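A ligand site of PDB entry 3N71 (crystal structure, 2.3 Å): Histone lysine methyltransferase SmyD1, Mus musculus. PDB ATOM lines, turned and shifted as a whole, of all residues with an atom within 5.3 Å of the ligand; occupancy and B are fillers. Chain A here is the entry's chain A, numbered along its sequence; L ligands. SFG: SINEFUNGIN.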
ATOM      1  N   GLY A  16     -13.616  36.250  21.638  1.00  0.00           N
ATOM      2  CA  GLY A  16     -14.283  35.615  20.521  1.00  0.00           C
ATOM      3  C   GLY A  16     -13.553  34.303  20.302  1.00  0.00           C
ATOM      4  O   GLY A  16     -13.780  33.580  19.325  1.00  0.00           O
ATOM      5  N   LYS A  17     -12.657  34.007  21.231  1.00  0.00           N
ATOM      6  CA  LYS A  17     -11.868  32.802  21.181  1.00  0.00           C
ATOM      7  C   LYS A  17     -12.545  31.680  21.951  1.00  0.00           C
ATOM      8  O   LYS A  17     -11.962  30.623  22.147  1.00  0.00           O
ATOM      9  CB  LYS A  17     -10.464  33.083  21.726  1.00  0.00           C
ATOM     10  CG  LYS A  17      -9.782  34.229  21.017  1.00  0.00           C
ATOM     11  CD  LYS A  17      -8.379  34.535  21.529  1.00  0.00           C
ATOM     12  CE  LYS A  17      -7.819  35.746  20.770  1.00  0.00           C
ATOM     13  NZ  LYS A  17      -6.542  36.278  21.335  1.00  0.00           N
ATOM     14  N   GLY A  18     -13.773  31.915  22.388  1.00  0.00           N
ATOM     15  CA  GLY A  18     -14.493  30.910  23.142  1.00  0.00           C
ATOM     16  C   GLY A  18     -13.750  30.547  24.423  1.00  0.00           C
ATOM     17  O   GLY A  18     -13.226  31.411  25.108  1.00  0.00           O
ATOM     18  N   ARG A  19     -13.698  29.267  24.736  1.00  0.00           N
ATOM     19  CA  ARG A  19     -13.004  28.824  25.941  1.00  0.00           C
ATOM     20  C   ARG A  19     -11.489  28.816  25.765  1.00  0.00           C
ATOM     21  O   ARG A  19     -10.979  28.660  24.650  1.00  0.00           O
ATOM     22  CB  ARG A  19     -13.473  27.439  26.348  1.00  0.00           C
ATOM     23  CG  ARG A  19     -14.867  27.426  26.919  1.00  0.00           C
ATOM     24  CD  ARG A  19     -15.295  26.003  27.196  1.00  0.00           C
ATOM     25  NE  ARG A  19     -15.537  25.296  25.945  1.00  0.00           N
ATOM     26  CZ  ARG A  19     -15.789  23.992  25.874  1.00  0.00           C
ATOM     27  NH1 ARG A  19     -15.824  23.259  26.972  1.00  0.00           N
ATOM     28  NH2 ARG A  19     -16.014  23.429  24.684  1.00  0.00           N
ATOM     29  N   GLY A  20     -10.782  28.964  26.887  1.00  0.00           N
ATOM     30  CA  GLY A  20      -9.339  28.957  26.897  1.00  0.00           C
ATOM     31  C   GLY A  20      -8.828  28.476  28.244  1.00  0.00           C
ATOM     32  O   GLY A  20      -9.608  28.230  29.161  1.00  0.00           O
ATOM     33  N   LEU A 132     -16.302  19.073  23.349  1.00  0.00           N
ATOM     34  CA  LEU A 132     -15.198  19.734  22.654  1.00  0.00           C
ATOM     35  C   LEU A 132     -15.787  20.518  21.486  1.00  0.00           C
ATOM     36  O   LEU A 132     -16.917  20.278  21.071  1.00  0.00           O
ATOM     37  CB  LEU A 132     -14.183  18.700  22.162  1.00  0.00           C
ATOM     38  CG  LEU A 132     -13.338  18.039  23.261  1.00  0.00           C
ATOM     39  CD1 LEU A 132     -12.639  16.784  22.714  1.00  0.00           C
ATOM     40  CD2 LEU A 132     -12.334  19.066  23.820  1.00  0.00           C
ATOM     41  N   GLN A 133     -15.026  21.467  20.946  1.00  0.00           N
ATOM     42  CA  GLN A 133     -15.568  22.256  19.857  1.00  0.00           C
ATOM     43  C   GLN A 133     -15.768  21.433  18.588  1.00  0.00           C
ATOM     44  O   GLN A 133     -14.993  20.526  18.284  1.00  0.00           O
ATOM     45  CB  GLN A 133     -14.667  23.463  19.592  1.00  0.00           C
ATOM     46  CG  GLN A 133     -15.416  24.622  18.948  1.00  0.00           C
ATOM     47  CD  GLN A 133     -14.644  25.940  19.007  1.00  0.00           C
ATOM     48  OE1 GLN A 133     -14.312  26.425  20.092  1.00  0.00           O
ATOM     49  NE2 GLN A 133     -14.358  26.498  17.852  1.00  0.00           N
ATOM     50  N   HIS A 135     -16.873  22.284  14.560  1.00  0.00           N
ATOM     51  CA  HIS A 135     -17.242  23.242  13.541  1.00  0.00           C
ATOM     52  C   HIS A 135     -18.002  22.604  12.382  1.00  0.00           C
ATOM     53  O   HIS A 135     -17.925  23.087  11.253  1.00  0.00           O
ATOM     54  CB  HIS A 135     -15.996  23.933  13.008  1.00  0.00           C
ATOM     55  CG  HIS A 135     -15.430  24.936  13.957  1.00  0.00           C
ATOM     56  ND1 HIS A 135     -16.167  26.008  14.421  1.00  0.00           N
ATOM     57  CD2 HIS A 135     -14.205  25.051  14.518  1.00  0.00           C
ATOM     58  CE1 HIS A 135     -15.417  26.731  15.231  1.00  0.00           C
ATOM     59  NE2 HIS A 135     -14.222  26.175  15.311  1.00  0.00           N
ATOM     60  N   CYS A 179     -12.128  18.352  14.260  1.00  0.00           N
ATOM     61  CA  CYS A 179     -11.683  19.634  14.794  1.00  0.00           C
ATOM     62  C   CYS A 179     -10.875  19.501  16.090  1.00  0.00           C
ATOM     63  O   CYS A 179     -10.672  20.505  16.788  1.00  0.00           O
ATOM     64  CB  CYS A 179     -12.898  20.551  15.032  1.00  0.00           C
ATOM     65  SG  CYS A 179     -14.024  20.773  13.598  1.00  0.00           S
ATOM     66  N   ASN A 180     -10.428  18.292  16.418  1.00  0.00           N
ATOM     67  CA  ASN A 180      -9.692  18.073  17.676  1.00  0.00           C
ATOM     68  C   ASN A 180      -8.642  16.962  17.733  1.00  0.00           C
ATOM     69  O   ASN A 180      -8.047  16.739  18.784  1.00  0.00           O
ATOM     70  CB  ASN A 180     -10.679  17.803  18.828  1.00  0.00           C
ATOM     71  CG  ASN A 180     -11.470  19.024  19.235  1.00  0.00           C
ATOM     72  OD1 ASN A 180     -10.965  19.910  19.935  1.00  0.00           O
ATOM     73  ND2 ASN A 180     -12.729  19.073  18.817  1.00  0.00           N
ATOM     74  N   LEU A 201      -6.175  19.144  26.321  1.00  0.00           N
ATOM     75  CA  LEU A 201      -5.376  19.885  25.351  1.00  0.00           C
ATOM     76  C   LEU A 201      -6.359  20.587  24.412  1.00  0.00           C
ATOM     77  O   LEU A 201      -6.041  21.628  23.840  1.00  0.00           O
ATOM     78  CB  LEU A 201      -4.467  18.938  24.576  1.00  0.00           C
ATOM     79  CG  LEU A 201      -3.435  19.489  23.588  1.00  0.00           C
ATOM     80  CD1 LEU A 201      -4.063  19.742  22.219  1.00  0.00           C
ATOM     81  CD2 LEU A 201      -2.838  20.766  24.157  1.00  0.00           C
ATOM     82  N   GLY A 202      -7.559  20.012  24.277  1.00  0.00           N
ATOM     83  CA  GLY A 202      -8.576  20.588  23.402  1.00  0.00           C
ATOM     84  C   GLY A 202      -9.125  21.957  23.799  1.00  0.00           C
ATOM     85  O   GLY A 202      -9.863  22.603  23.029  1.00  0.00           O
ATOM     86  N   LEU A 203      -8.769  22.417  24.999  1.00  0.00           N
ATOM     87  CA  LEU A 203      -9.230  23.697  25.474  1.00  0.00           C
ATOM     88  C   LEU A 203      -8.212  24.811  25.246  1.00  0.00           C
ATOM     89  O   LEU A 203      -8.511  25.985  25.497  1.00  0.00           O
ATOM     90  CB  LEU A 203      -9.572  23.621  26.960  1.00  0.00           C
ATOM     91  CG  LEU A 203     -10.902  22.952  27.341  1.00  0.00           C
ATOM     92  CD1 LEU A 203     -11.004  21.575  26.716  1.00  0.00           C
ATOM     93  CD2 LEU A 203     -11.016  22.853  28.861  1.00  0.00           C
ATOM     94  N   VAL A 204      -7.021  24.455  24.764  1.00  0.00           N
ATOM     95  CA  VAL A 204      -5.989  25.457  24.544  1.00  0.00           C
ATOM     96  C   VAL A 204      -6.081  26.150  23.185  1.00  0.00           C
ATOM     97  O   VAL A 204      -6.147  25.496  22.140  1.00  0.00           O
ATOM     98  CB  VAL A 204      -4.589  24.846  24.695  1.00  0.00           C
ATOM     99  CG1 VAL A 204      -3.522  25.911  24.445  1.00  0.00           C
ATOM    100  CG2 VAL A 204      -4.431  24.283  26.104  1.00  0.00           C
ATOM    101  N   ASN A 205      -6.096  27.488  23.203  1.00  0.00           N
ATOM    102  CA  ASN A 205      -6.172  28.272  21.982  1.00  0.00           C
ATOM    103  C   ASN A 205      -4.847  28.478  21.250  1.00  0.00           C
ATOM    104  O   ASN A 205      -3.763  28.261  21.792  1.00  0.00           O
ATOM    105  CB  ASN A 205      -6.798  29.654  22.262  1.00  0.00           C
ATOM    106  CG  ASN A 205      -8.274  29.563  22.523  1.00  0.00           C
ATOM    107  OD1 ASN A 205      -9.000  28.850  21.840  1.00  0.00           O
ATOM    108  ND2 ASN A 205      -8.737  30.310  23.524  1.00  0.00           N
ATOM    109  N   HIS A 206      -4.965  28.962  20.015  1.00  0.00           N
ATOM    110  CA  HIS A 206      -3.830  29.187  19.143  1.00  0.00           C
ATOM    111  C   HIS A 206      -3.221  30.576  19.161  1.00  0.00           C
ATOM    112  O   HIS A 206      -3.877  31.582  19.409  1.00  0.00           O
ATOM    113  CB  HIS A 206      -4.246  28.858  17.702  1.00  0.00           C
ATOM    114  CG  HIS A 206      -3.239  29.282  16.677  1.00  0.00           C
ATOM    115  ND1 HIS A 206      -2.169  28.502  16.317  1.00  0.00           N
ATOM    116  CD2 HIS A 206      -3.057  30.476  16.044  1.00  0.00           C
ATOM    117  CE1 HIS A 206      -1.360  29.191  15.528  1.00  0.00           C
ATOM    118  NE2 HIS A 206      -1.880  30.402  15.350  1.00  0.00           N
ATOM    119  N   ASP A 207      -1.923  30.616  18.876  1.00  0.00           N
ATOM    120  CA  ASP A 207      -1.158  31.852  18.762  1.00  0.00           C
ATOM    121  C   ASP A 207       0.060  31.460  17.903  1.00  0.00           C
ATOM    122  O   ASP A 207       0.706  30.445  18.157  1.00  0.00           O
ATOM    123  CB  ASP A 207      -0.708  32.357  20.133  1.00  0.00           C
ATOM    124  CG  ASP A 207      -0.156  33.783  20.062  1.00  0.00           C
ATOM    125  OD1 ASP A 207       0.673  34.075  19.173  1.00  0.00           O
ATOM    126  OD2 ASP A 207      -0.547  34.614  20.919  1.00  0.00           O
ATOM    127  N   TYR A 252      -0.985  25.946  16.241  1.00  0.00           N
ATOM    128  CA  TYR A 252      -1.646  24.877  15.514  1.00  0.00           C
ATOM    129  C   TYR A 252      -0.914  24.594  14.208  1.00  0.00           C
ATOM    130  O   TYR A 252      -1.097  23.538  13.613  1.00  0.00           O
ATOM    131  CB  TYR A 252      -3.091  25.269  15.165  1.00  0.00           C
ATOM    132  CG  TYR A 252      -4.058  25.417  16.339  1.00  0.00           C
ATOM    133  CD1 TYR A 252      -3.619  25.377  17.656  1.00  0.00           C
ATOM    134  CD2 TYR A 252      -5.423  25.615  16.109  1.00  0.00           C
ATOM    135  CE1 TYR A 252      -4.507  25.538  18.720  1.00  0.00           C
ATOM    136  CE2 TYR A 252      -6.314  25.786  17.160  1.00  0.00           C
ATOM    137  CZ  TYR A 252      -5.856  25.748  18.465  1.00  0.00           C
ATOM    138  OH  TYR A 252      -6.730  25.956  19.517  1.00  0.00           O
ATOM    139  N   TYR A 270      -9.233  25.760  10.947  1.00  0.00           N
ATOM    140  CA  TYR A 270      -9.848  26.041  12.247  1.00  0.00           C
ATOM    141  C   TYR A 270     -10.918  27.132  12.293  1.00  0.00           C
ATOM    142  O   TYR A 270     -11.224  27.681  13.358  1.00  0.00           O
ATOM    143  CB  TYR A 270      -8.763  26.365  13.260  1.00  0.00           C
ATOM    144  CG  TYR A 270      -7.789  25.232  13.404  1.00  0.00           C
ATOM    145  CD1 TYR A 270      -8.137  24.076  14.107  1.00  0.00           C
ATOM    146  CD2 TYR A 270      -6.527  25.298  12.829  1.00  0.00           C
ATOM    147  CE1 TYR A 270      -7.257  23.014  14.220  1.00  0.00           C
ATOM    148  CE2 TYR A 270      -5.618  24.232  12.939  1.00  0.00           C
ATOM    149  CZ  TYR A 270      -6.001  23.101  13.640  1.00  0.00           C
ATOM    150  OH  TYR A 270      -5.117  22.052  13.770  1.00  0.00           O
ATOM    151  N   TYR A 271     -11.473  27.451  11.125  1.00  0.00           N
ATOM    152  CA  TYR A 271     -12.511  28.463  11.011  1.00  0.00           C
ATOM    153  C   TYR A 271     -12.393  29.703  11.892  1.00  0.00           C
ATOM    154  O   TYR A 271     -13.333  30.028  12.627  1.00  0.00           O
ATOM    155  CB  TYR A 271     -13.884  27.820  11.239  1.00  0.00           C
ATOM    156  CG  TYR A 271     -14.087  26.565  10.424  1.00  0.00           C
ATOM    157  CD1 TYR A 271     -13.672  25.325  10.901  1.00  0.00           C
ATOM    158  CD2 TYR A 271     -14.654  26.623   9.150  1.00  0.00           C
ATOM    159  CE1 TYR A 271     -13.816  24.171  10.138  1.00  0.00           C
ATOM    160  CE2 TYR A 271     -14.797  25.470   8.373  1.00  0.00           C
ATOM    161  CZ  TYR A 271     -14.385  24.250   8.882  1.00  0.00           C
ATOM    162  OH  TYR A 271     -14.515  23.093   8.135  1.00  0.00           O
ATOM    163  N   PHE A 272     -11.263  30.397  11.833  1.00  0.00           N
ATOM    164  CA  PHE A 272     -11.118  31.627  12.593  1.00  0.00           C
ATOM    165  C   PHE A 272     -10.053  32.536  12.002  1.00  0.00           C
ATOM    166  O   PHE A 272      -9.200  32.088  11.251  1.00  0.00           O
ATOM    167  CB  PHE A 272     -10.814  31.347  14.072  1.00  0.00           C
ATOM    168  CG  PHE A 272      -9.396  30.988  14.364  1.00  0.00           C
ATOM    169  CD1 PHE A 272      -8.983  29.658  14.416  1.00  0.00           C
ATOM    170  CD2 PHE A 272      -8.446  31.979  14.629  1.00  0.00           C
ATOM    171  CE1 PHE A 272      -7.666  29.324  14.734  1.00  0.00           C
ATOM    172  CE2 PHE A 272      -7.136  31.653  14.947  1.00  0.00           C
ATOM    173  CZ  PHE A 272      -6.734  30.315  14.996  1.00  0.00           C
ATOM    174  N   ASP A 273     -10.151  33.824  12.326  1.00  0.00           N
ATOM    175  CA  ASP A 273      -9.180  34.808  11.835  1.00  0.00           C
ATOM    176  C   ASP A 273      -8.191  35.095  12.951  1.00  0.00           C
ATOM    177  O   ASP A 273      -8.520  35.743  13.934  1.00  0.00           O
ATOM    178  CB  ASP A 273      -9.893  36.104  11.412  1.00  0.00           C
ATOM    179  CG  ASP A 273     -11.049  35.862  10.459  1.00  0.00           C
ATOM    180  OD1 ASP A 273     -10.886  35.058   9.517  1.00  0.00           O
ATOM    181  OD2 ASP A 273     -12.118  36.492  10.667  1.00  0.00           O
ATOM    182  N   CYS A 274      -6.964  34.612  12.795  1.00  0.00           N
ATOM    183  CA  CYS A 274      -5.971  34.821  13.828  1.00  0.00           C
ATOM    184  C   CYS A 274      -5.656  36.294  14.092  1.00  0.00           C
ATOM    185  O   CYS A 274      -5.412  37.068  13.174  1.00  0.00           O
ATOM    186  CB  CYS A 274      -4.684  34.084  13.461  1.00  0.00           C
ATOM    187  SG  CYS A 274      -3.501  34.141  14.801  1.00  0.00           S
ATOM    188  N   SER A 275      -5.632  36.661  15.370  1.00  0.00           N
ATOM    189  CA  SER A 275      -5.373  38.041  15.735  1.00  0.00           C
ATOM    190  C   SER A 275      -4.207  38.180  16.695  1.00  0.00           C
ATOM    191  O   SER A 275      -4.167  39.136  17.479  1.00  0.00           O
ATOM    192  CB  SER A 275      -6.616  38.660  16.372  1.00  0.00           C
ATOM    193  OG  SER A 275      -6.937  37.964  17.558  1.00  0.00           O
HETATM  194  N   SFG L   1     -11.742  27.879  22.206  1.00  0.00           N
HETATM  195  CA  SFG L   1     -11.969  26.406  22.192  1.00  0.00           C
HETATM  196  C   SFG L   1     -13.145  25.833  23.042  1.00  0.00           C
HETATM  197  O   SFG L   1     -13.230  24.606  23.294  1.00  0.00           O
HETATM  198  OXT SFG L   1     -14.023  26.587  23.482  1.00  0.00           O
HETATM  199  CB  SFG L   1     -10.587  25.783  22.563  1.00  0.00           C
HETATM  200  CG  SFG L   1      -9.720  25.333  21.359  1.00  0.00           C
HETATM  201  CD  SFG L   1     -10.366  24.353  20.315  1.00  0.00           C
HETATM  202  NE  SFG L   1      -9.562  23.096  20.287  1.00  0.00           N
HETATM  203  C5' SFG L   1     -10.388  24.783  18.839  1.00  0.00           C
HETATM  204  C4' SFG L   1     -11.155  26.055  18.384  1.00  0.00           C
HETATM  205  O4' SFG L   1     -10.930  27.254  19.157  1.00  0.00           O
HETATM  206  C3' SFG L   1     -10.814  26.481  16.979  1.00  0.00           C
HETATM  207  O3' SFG L   1     -11.409  25.644  16.000  1.00  0.00           O
HETATM  208  C2' SFG L   1     -11.305  27.916  16.910  1.00  0.00           C
HETATM  209  O2' SFG L   1     -12.706  27.957  16.587  1.00  0.00           O
HETATM  210  C1' SFG L   1     -11.011  28.419  18.311  1.00  0.00           C
HETATM  211  N9  SFG L   1      -9.732  29.186  18.406  1.00  0.00           N
HETATM  212  C8  SFG L   1      -8.480  28.684  18.712  1.00  0.00           C
HETATM  213  N7  SFG L   1      -7.565  29.604  18.708  1.00  0.00           N
HETATM  214  C5  SFG L   1      -8.232  30.791  18.405  1.00  0.00           C
HETATM  215  C6  SFG L   1      -7.826  32.169  18.205  1.00  0.00           C
HETATM  216  N6  SFG L   1      -6.559  32.643  18.363  1.00  0.00           N
HETATM  217  N1  SFG L   1      -8.784  33.126  17.886  1.00  0.00           N
HETATM  218  C2  SFG L   1     -10.062  32.707  17.727  1.00  0.00           C
HETATM  219  N3  SFG L   1     -10.558  31.451  17.875  1.00  0.00           N
HETATM  220  C4  SFG L   1      -9.584  30.531  18.173  1.00  0.00           C
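N of Tyr 252 sits at hydrogen-bond distance from ND1 of His 206 (2.8 Å). ND2 of Asn 180 lies within hydrogen-bond range of O of Gln 133, at 2.7 Å. A ring nitrogen (NE2) of His 135 sits at hydrogen-bond distance from the side-chain amide nitrogen (NE2) of Gln 133 (2.6 Å). The backbone carbonyl oxygen of Lys 17 sits close to the side-chain amide oxygen of Asn 205. The backbone NH of His 135 is in hydrogen-bond range of the side-chain sulfur of Cys 179 (3.4 Å). The side-chain amide nitrogen (ND2) of Asn 205 sits at hydrogen-bond distance from the backbone carbonyl oxygen (O) of Arg 19. The side-chain hydroxyl (OH) of Tyr 252 lies within hydrogen-bond range of the backbone carbonyl oxygen (O) of Val 204, 2.7 Å away.
Residues that only touch the ligand: Leu 203, Val 204, Tyr 252 and Phe 272. Hydrophobic or aromatic side chains that line the ligand: His 135, His 206, Tyr 252, Tyr 270 and Phe 272. Within 4 Å of the ligand: Lys 17, Arg 19, Gln 133, His 135, Asn 180, Gly 202, Leu 203, Val 204, Asn 205, His 206, Tyr 252, Tyr 270 and Phe 272. The nearest printed residue that does not touch the ligand is Gly 18 (4.01 Å).
O of Tyr 270 lies within hydrogen-bond range of O3' of the ligand (3.3 Å). A nitrogen (NE) of the ligand lies within hydrogen-bond range of the backbone carbonyl oxygen (O) of Gly 202, 2.8 Å away. The backbone carbonyl oxygen of Lys 17 sits at hydrogen-bond distance from a nitrogen (N) of the ligand. OXT of the ligand lies within salt-bridge range of NE of Arg 19 (3.2 Å). A nitrogen (N) of the ligand is in hydrogen-bond range of the backbone carbonyl oxygen of Arg 19 (2.7 Å). The side-chain amide oxygen (OD1) of Asn 205 lies within hydrogen-bond range of a nitrogen (N) of the ligand. The backbone NH of Arg 19 lies within hydrogen-bond range of an oxygen (OXT) of the ligand (3.0 Å). The backbone carbonyl oxygen (O) of His 206 lies within hydrogen-bond range of a nitrogen (N6) of the ligand. The side-chain amide oxygen (OD1) of Asn 180 sits at hydrogen-bond distance from a nitrogen (NE) of the ligand (3.5 Å). N of His 206 is in hydrogen-bond range of N7 of the ligand, at 3.0 Å. O2' of the ligand sits at hydrogen-bond distance from NE2 of Gln 133, at 2.5 Å. An oxygen (O2') of the ligand lies within hydrogen-bond range of a ring nitrogen (NE2) of His 135.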
